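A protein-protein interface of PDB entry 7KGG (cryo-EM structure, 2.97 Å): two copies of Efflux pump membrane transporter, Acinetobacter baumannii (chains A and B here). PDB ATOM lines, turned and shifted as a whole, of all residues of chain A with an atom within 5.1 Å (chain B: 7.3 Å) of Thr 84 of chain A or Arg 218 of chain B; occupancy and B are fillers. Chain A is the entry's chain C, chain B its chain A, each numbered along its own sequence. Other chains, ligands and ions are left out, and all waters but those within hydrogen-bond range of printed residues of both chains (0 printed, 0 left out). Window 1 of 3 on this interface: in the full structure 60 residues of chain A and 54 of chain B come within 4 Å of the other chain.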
ATOM      1  N   ALA A  52     -27.438 -20.543  13.438  1.00  0.00           N
ATOM      2  CA  ALA A  52     -28.147 -20.802  12.195  1.00  0.00           C
ATOM      3  C   ALA A  52     -28.710 -19.517  11.602  1.00  0.00           C
ATOM      4  O   ALA A  52     -28.942 -18.528  12.302  1.00  0.00           O
ATOM      5  CB  ALA A  52     -29.279 -21.799  12.423  1.00  0.00           C
ATOM      6  N   ALA A  54     -31.589 -17.150   9.626  1.00  0.00           N
ATOM      7  CA  ALA A  54     -33.007 -16.936   9.897  1.00  0.00           C
ATOM      8  C   ALA A  54     -33.868 -17.918   9.114  1.00  0.00           C
ATOM      9  O   ALA A  54     -34.907 -18.375   9.606  1.00  0.00           O
ATOM     10  CB  ALA A  54     -33.393 -15.497   9.561  1.00  0.00           C
ATOM     11  N   THR A  82     -38.374 -14.209  13.090  1.00  0.00           N
ATOM     12  CA  THR A  82     -37.057 -14.822  13.178  1.00  0.00           C
ATOM     13  C   THR A  82     -36.015 -13.831  12.682  1.00  0.00           C
ATOM     14  O   THR A  82     -36.210 -13.176  11.654  1.00  0.00           O
ATOM     15  CB  THR A  82     -36.984 -16.114  12.352  1.00  0.00           C
ATOM     16  OG1 THR A  82     -37.960 -17.047  12.828  1.00  0.00           O
ATOM     17  CG2 THR A  82     -35.600 -16.741  12.448  1.00  0.00           C
ATOM     18  N   ASP A  83     -34.905 -13.737  13.415  1.00  0.00           N
ATOM     19  CA  ASP A  83     -33.817 -12.824  13.096  1.00  0.00           C
ATOM     20  C   ASP A  83     -32.524 -13.622  12.976  1.00  0.00           C
ATOM     21  O   ASP A  83     -32.491 -14.833  13.221  1.00  0.00           O
ATOM     22  CB  ASP A  83     -33.685 -11.727  14.160  1.00  0.00           C
ATOM     23  CG  ASP A  83     -34.731 -10.641  14.013  1.00  0.00           C
ATOM     24  OD1 ASP A  83     -34.731  -9.953  12.971  1.00  0.00           O
ATOM     25  OD2 ASP A  83     -35.548 -10.469  14.942  1.00  0.00           O
ATOM     26  N   THR A  84     -31.448 -12.932  12.593  1.00  0.00           N
ATOM     27  CA  THR A  84     -30.140 -13.565  12.485  1.00  0.00           C
ATOM     28  C   THR A  84     -29.518 -13.870  13.842  1.00  0.00           C
ATOM     29  O   THR A  84     -28.530 -14.608  13.896  1.00  0.00           O
ATOM     30  CB  THR A  84     -29.186 -12.674  11.684  1.00  0.00           C
ATOM     31  OG1 THR A  84     -29.069 -11.396  12.321  1.00  0.00           O
ATOM     32  CG2 THR A  84     -29.684 -12.490  10.257  1.00  0.00           C
ATOM     33  N   SER A  85     -30.068 -13.326  14.930  1.00  0.00           N
ATOM     34  CA  SER A  85     -29.509 -13.575  16.252  1.00  0.00           C
ATOM     35  C   SER A  85     -29.655 -15.030  16.679  1.00  0.00           C
ATOM     36  O   SER A  85     -28.992 -15.452  17.633  1.00  0.00           O
ATOM     37  CB  SER A  85     -30.178 -12.665  17.284  1.00  0.00           C
ATOM     38  OG  SER A  85     -31.583 -12.643  17.107  1.00  0.00           O
ATOM     39  N   GLY A  86     -30.502 -15.801  16.002  1.00  0.00           N
ATOM     40  CA  GLY A  86     -30.706 -17.196  16.326  1.00  0.00           C
ATOM     41  C   GLY A  86     -31.910 -17.481  17.196  1.00  0.00           C
ATOM     42  O   GLY A  86     -32.079 -18.628  17.629  1.00  0.00           O
ATOM     43  N   SER A 577     -26.575  -3.512   7.618  1.00  0.00           N
ATOM     44  CA  SER A 577     -26.472  -4.929   7.956  1.00  0.00           C
ATOM     45  C   SER A 577     -25.055  -5.305   8.374  1.00  0.00           C
ATOM     46  O   SER A 577     -24.863  -6.040   9.350  1.00  0.00           O
ATOM     47  CB  SER A 577     -26.920  -5.780   6.769  1.00  0.00           C
ATOM     48  OG  SER A 577     -27.220  -7.104   7.175  1.00  0.00           O
ATOM     49  N   ALA A 615     -33.368  -7.920  16.363  1.00  0.00           N
ATOM     50  CA  ALA A 615     -32.193  -8.031  17.212  1.00  0.00           C
ATOM     51  C   ALA A 615     -30.965  -8.281  16.351  1.00  0.00           C
ATOM     52  O   ALA A 615     -31.024  -9.023  15.365  1.00  0.00           O
ATOM     53  CB  ALA A 615     -32.351  -9.158  18.238  1.00  0.00           C
ATOM     54  N   GLN A 617     -26.463  -6.771  15.805  1.00  0.00           N
ATOM     55  CA  GLN A 617     -25.363  -5.870  16.225  1.00  0.00           C
ATOM     56  C   GLN A 617     -25.525  -4.506  15.568  1.00  0.00           C
ATOM     57  O   GLN A 617     -24.709  -3.636  15.864  1.00  0.00           O
ATOM     58  CB  GLN A 617     -24.016  -6.496  15.868  1.00  0.00           C
ATOM     59  CG  GLN A 617     -23.870  -7.957  16.263  1.00  0.00           C
ATOM     60  CD  GLN A 617     -22.507  -8.499  15.905  1.00  0.00           C
ATOM     61  OE1 GLN A 617     -21.509  -7.786  15.925  1.00  0.00           O
ATOM     62  NE2 GLN A 617     -22.453  -9.777  15.576  1.00  0.00           N
ATOM     63  N   MET A 745     -17.374 -22.095  13.852  1.00  0.00           N
ATOM     64  CA  MET A 745     -18.101 -20.838  13.983  1.00  0.00           C
ATOM     65  C   MET A 745     -19.254 -20.901  14.974  1.00  0.00           C
ATOM     66  O   MET A 745     -20.055 -19.961  15.025  1.00  0.00           O
ATOM     67  CB  MET A 745     -18.636 -20.399  12.614  1.00  0.00           C
ATOM     68  CG  MET A 745     -17.557 -20.058  11.601  1.00  0.00           C
ATOM     69  SD  MET A 745     -16.563 -18.636  12.094  1.00  0.00           S
ATOM     70  CE  MET A 745     -15.285 -18.659  10.840  1.00  0.00           C
ATOM     71  N   ARG A 771     -11.765 -16.520  14.209  1.00  0.00           N
ATOM     72  CA  ARG A 771     -13.105 -16.660  13.649  1.00  0.00           C
ATOM     73  C   ARG A 771     -13.652 -15.312  13.190  1.00  0.00           C
ATOM     74  O   ARG A 771     -14.845 -15.025  13.325  1.00  0.00           O
ATOM     75  CB  ARG A 771     -14.040 -17.330  14.655  1.00  0.00           C
ATOM     76  CG  ARG A 771     -14.476 -16.461  15.827  1.00  0.00           C
ATOM     77  CD  ARG A 771     -15.368 -17.242  16.779  1.00  0.00           C
ATOM     78  NE  ARG A 771     -15.234 -16.788  18.160  1.00  0.00           N
ATOM     79  CZ  ARG A 771     -15.825 -15.706  18.658  1.00  0.00           C
ATOM     80  NH1 ARG A 771     -15.640 -15.378  19.929  1.00  0.00           N
ATOM     81  NH2 ARG A 771     -16.598 -14.950  17.892  1.00  0.00           N
ATOM     82  N   GLN A 805     -32.684 -10.664   6.088  1.00  0.00           N
ATOM     83  CA  GLN A 805     -32.089 -10.918   7.409  1.00  0.00           C
ATOM     84  C   GLN A 805     -33.204 -11.011   8.430  1.00  0.00           C
ATOM     85  O   GLN A 805     -32.869 -10.974   9.584  1.00  0.00           O
ATOM     86  CB  GLN A 805     -31.098  -9.818   7.768  1.00  0.00           C
ATOM     87  CG  GLN A 805     -31.713  -8.497   8.179  1.00  0.00           C
ATOM     88  CD  GLN A 805     -30.664  -7.533   8.665  1.00  0.00           C
ATOM     89  OE1 GLN A 805     -29.817  -7.865   9.493  1.00  0.00           O
ATOM     90  NE2 GLN A 805     -30.723  -6.315   8.165  1.00  0.00           N
ATOM     91  N   ALA B 215     -25.211 -25.730  10.753  1.00  0.00           N
ATOM     92  CA  ALA B 215     -25.497 -24.455  11.395  1.00  0.00           C
ATOM     93  C   ALA B 215     -24.257 -23.571  11.374  1.00  0.00           C
ATOM     94  O   ALA B 215     -23.584 -23.422  12.401  1.00  0.00           O
ATOM     95  CB  ALA B 215     -25.974 -24.672  12.832  1.00  0.00           C
ATOM     96  N   PRO B 216     -23.920 -22.967  10.232  1.00  0.00           N
ATOM     97  CA  PRO B 216     -22.790 -22.032  10.198  1.00  0.00           C
ATOM     98  C   PRO B 216     -23.081 -20.780  11.009  1.00  0.00           C
ATOM     99  O   PRO B 216     -24.202 -20.267  11.036  1.00  0.00           O
ATOM    100  CB  PRO B 216     -22.651 -21.703   8.702  1.00  0.00           C
ATOM    101  CG  PRO B 216     -23.490 -22.722   7.983  1.00  0.00           C
ATOM    102  CD  PRO B 216     -24.587 -23.058   8.926  1.00  0.00           C
ATOM    103  N   GLY B 217     -22.044 -20.269  11.663  1.00  0.00           N
ATOM    104  CA  GLY B 217     -22.213 -19.126  12.536  1.00  0.00           C
ATOM    105  C   GLY B 217     -22.138 -17.808  11.798  1.00  0.00           C
ATOM    106  O   GLY B 217     -22.829 -17.609  10.795  1.00  0.00           O
ATOM    107  N   ARG B 218     -21.299 -16.899  12.286  1.00  0.00           N
ATOM    108  CA  ARG B 218     -21.139 -15.585  11.684  1.00  0.00           C
ATOM    109  C   ARG B 218     -19.676 -15.178  11.760  1.00  0.00           C
ATOM    110  O   ARG B 218     -18.957 -15.562  12.686  1.00  0.00           O
ATOM    111  CB  ARG B 218     -22.000 -14.530  12.394  1.00  0.00           C
ATOM    112  CG  ARG B 218     -23.499 -14.734  12.264  1.00  0.00           C
ATOM    113  CD  ARG B 218     -24.255 -13.532  12.807  1.00  0.00           C
ATOM    114  NE  ARG B 218     -24.299 -12.431  11.848  1.00  0.00           N
ATOM    115  CZ  ARG B 218     -24.894 -11.264  12.074  1.00  0.00           C
ATOM    116  NH1 ARG B 218     -24.882 -10.323  11.139  1.00  0.00           N
ATOM    117  NH2 ARG B 218     -25.498 -11.032  13.232  1.00  0.00           N
ATOM    118  N   LEU B 219     -19.241 -14.399  10.773  1.00  0.00           N
ATOM    119  CA  LEU B 219     -17.934 -13.760  10.822  1.00  0.00           C
ATOM    120  C   LEU B 219     -18.058 -12.468  11.619  1.00  0.00           C
ATOM    121  O   LEU B 219     -18.929 -11.640  11.336  1.00  0.00           O
ATOM    122  CB  LEU B 219     -17.409 -13.473   9.415  1.00  0.00           C
ATOM    123  CG  LEU B 219     -17.243 -14.679   8.485  1.00  0.00           C
ATOM    124  CD1 LEU B 219     -16.935 -14.215   7.071  1.00  0.00           C
ATOM    125  CD2 LEU B 219     -16.157 -15.622   8.983  1.00  0.00           C
ATOM    126  N   GLY B 220     -17.197 -12.306  12.618  1.00  0.00           N
ATOM    127  CA  GLY B 220     -17.291 -11.175  13.517  1.00  0.00           C
ATOM    128  C   GLY B 220     -18.286 -11.340  14.643  1.00  0.00           C
ATOM    129  O   GLY B 220     -18.625 -10.346  15.296  1.00  0.00           O
ATOM    130  N   ASP B 221     -18.766 -12.556  14.891  1.00  0.00           N
ATOM    131  CA  ASP B 221     -19.768 -12.776  15.924  1.00  0.00           C
ATOM    132  C   ASP B 221     -19.218 -12.403  17.293  1.00  0.00           C
ATOM    133  O   ASP B 221     -18.042 -12.626  17.592  1.00  0.00           O
ATOM    134  CB  ASP B 221     -20.215 -14.237  15.923  1.00  0.00           C
ATOM    135  CG  ASP B 221     -21.404 -14.485  16.831  1.00  0.00           C
ATOM    136  OD1 ASP B 221     -21.866 -13.530  17.488  1.00  0.00           O
ATOM    137  OD2 ASP B 221     -21.878 -15.639  16.887  1.00  0.00           O
ATOM    138  N   LEU B 222     -20.079 -11.830  18.129  1.00  0.00           N
ATOM    139  CA  LEU B 222     -19.662 -11.439  19.465  1.00  0.00           C
ATOM    140  C   LEU B 222     -19.386 -12.681  20.313  1.00  0.00           C
ATOM    141  O   LEU B 222     -20.125 -13.667  20.227  1.00  0.00           O
ATOM    142  CB  LEU B 222     -20.739 -10.584  20.132  1.00  0.00           C
ATOM    143  CG  LEU B 222     -21.068  -9.244  19.468  1.00  0.00           C
ATOM    144  CD1 LEU B 222     -21.909  -8.391  20.404  1.00  0.00           C
ATOM    145  CD2 LEU B 222     -19.807  -8.498  19.053  1.00  0.00           C
ATOM    146  N   THR B 231     -19.547  -7.664   9.713  1.00  0.00           N
ATOM    147  CA  THR B 231     -20.106  -8.918  10.199  1.00  0.00           C
ATOM    148  C   THR B 231     -21.099  -9.429   9.167  1.00  0.00           C
ATOM    149  O   THR B 231     -21.954  -8.670   8.698  1.00  0.00           O
ATOM    150  CB  THR B 231     -20.784  -8.742  11.566  1.00  0.00           C
ATOM    151  OG1 THR B 231     -21.067 -10.027  12.133  1.00  0.00           O
ATOM    152  CG2 THR B 231     -22.078  -7.947  11.435  1.00  0.00           C
ATOM    153  N   ILE B 232     -20.980 -10.703   8.807  1.00  0.00           N
ATOM    154  CA  ILE B 232     -21.807 -11.280   7.751  1.00  0.00           C
ATOM    155  C   ILE B 232     -22.204 -12.703   8.133  1.00  0.00           C
ATOM    156  O   ILE B 232     -21.345 -13.488   8.562  1.00  0.00           O
ATOM    157  CB  ILE B 232     -21.071 -11.251   6.401  1.00  0.00           C
ATOM    158  CG1 ILE B 232     -22.013 -11.668   5.272  1.00  0.00           C
ATOM    159  CG2 ILE B 232     -19.849 -12.156   6.437  1.00  0.00           C
ATOM    160  CD1 ILE B 232     -21.541 -11.237   3.901  1.00  0.00           C
ATOM    161  N   PRO B 233     -23.475 -13.083   8.007  1.00  0.00           N
ATOM    162  CA  PRO B 233     -23.860 -14.465   8.313  1.00  0.00           C
ATOM    163  C   PRO B 233     -23.267 -15.461   7.329  1.00  0.00           C
ATOM    164  O   PRO B 233     -22.842 -15.108   6.227  1.00  0.00           O
ATOM    165  CB  PRO B 233     -25.390 -14.435   8.214  1.00  0.00           C
ATOM    166  CG  PRO B 233     -25.749 -13.022   8.485  1.00  0.00           C
ATOM    167  CD  PRO B 233     -24.663 -12.230   7.824  1.00  0.00           C
ATOM    168  N   LEU B 234     -23.248 -16.723   7.750  1.00  0.00           N
ATOM    169  CA  LEU B 234     -22.758 -17.831   6.942  1.00  0.00           C
ATOM    170  C   LEU B 234     -23.878 -18.840   6.738  1.00  0.00           C
ATOM    171  O   LEU B 234     -24.640 -19.131   7.667  1.00  0.00           O
ATOM    172  CB  LEU B 234     -21.558 -18.514   7.609  1.00  0.00           C
ATOM    173  CG  LEU B 234     -20.206 -17.811   7.463  1.00  0.00           C
ATOM    174  CD1 LEU B 234     -19.200 -18.390   8.444  1.00  0.00           C
ATOM    175  CD2 LEU B 234     -19.690 -17.926   6.039  1.00  0.00           C
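The backbone carbonyl oxygen of Gly 217 of chain B sits at hydrogen-bond distance from the backbone NH of Leu 234 of chain B.
OG1 of Thr 231 of chain B sits at hydrogen-bond distance from O of Leu 219 of chain B.
O of Ile 232 of chain B is in hydrogen-bond range of N of Leu 219 of chain B, 3.2 Å away.
The guanidinium group (NH2) of Arg 771 of chain A sits at hydrogen-bond distance from the backbone carbonyl oxygen (O) of Asp 221 of chain B (2.8 Å).
Ser 85 of chain A touches none of the printed residues of chain B.
Printed residues of chain A within 4 Å of Arg 218 of chain B: Thr 84 and Met 745.
Of the printed residues of chain A, Leu 219 of chain B touches Met 745 (3.7 Å).
Printed residues of chain A within 4 Å of Gly 220 of chain B: Gln 617 and Arg 771.
Pro 233 of chain B touches none of the printed residues of chain A.
The nearest residue of chain B that does not touch Thr 84 of chain A is Pro 233 of chain B (4.3 Å).
The nearest residue of chain A that does not touch Arg 218 of chain B is Gln 617 of chain A (4.04 Å).
No position is printed for both chains.
Of the 11 pairs that touch across the chains among the printed residues, none has its exchanged pair printed and touching as well.
Hydrophobic or aromatic side chains of chain A that line the printed part of chain B: Met 745.
Among the printed residues, no Asp or Glu carboxylate lies within 4 Å of a Lys or Arg side-chain nitrogen of the other chain.
Arg 218 of chain B touches Thr 84 of chain A (NH2 to OG1, 3.7 Å).
CG2 of Thr 231 of chain B touches O of Ser 577 of chain A (3.97 Å).
Gln 617 of chain A touches Gly 220 of chain B.
OE1 of Gln 617 of chain A touches CD2 of Leu 222 of chain B, 3.6 Å away.
Gln 617 of chain A touches Thr 231 of chain B (NE2 to OG1, 3.7 Å).
Met 745 of chain A touches Gly 217 of chain B.
SD of Met 745 of chain A touches O of Arg 218 of chain B, 3.9 Å away.
Met 745 of chain A touches Leu 219 of chain B.
CG of Met 745 of chain A touches CD1 of Leu 234 of chain B, at 3.9 Å.
Gly 220 of chain B touches Arg 771 of chain A.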
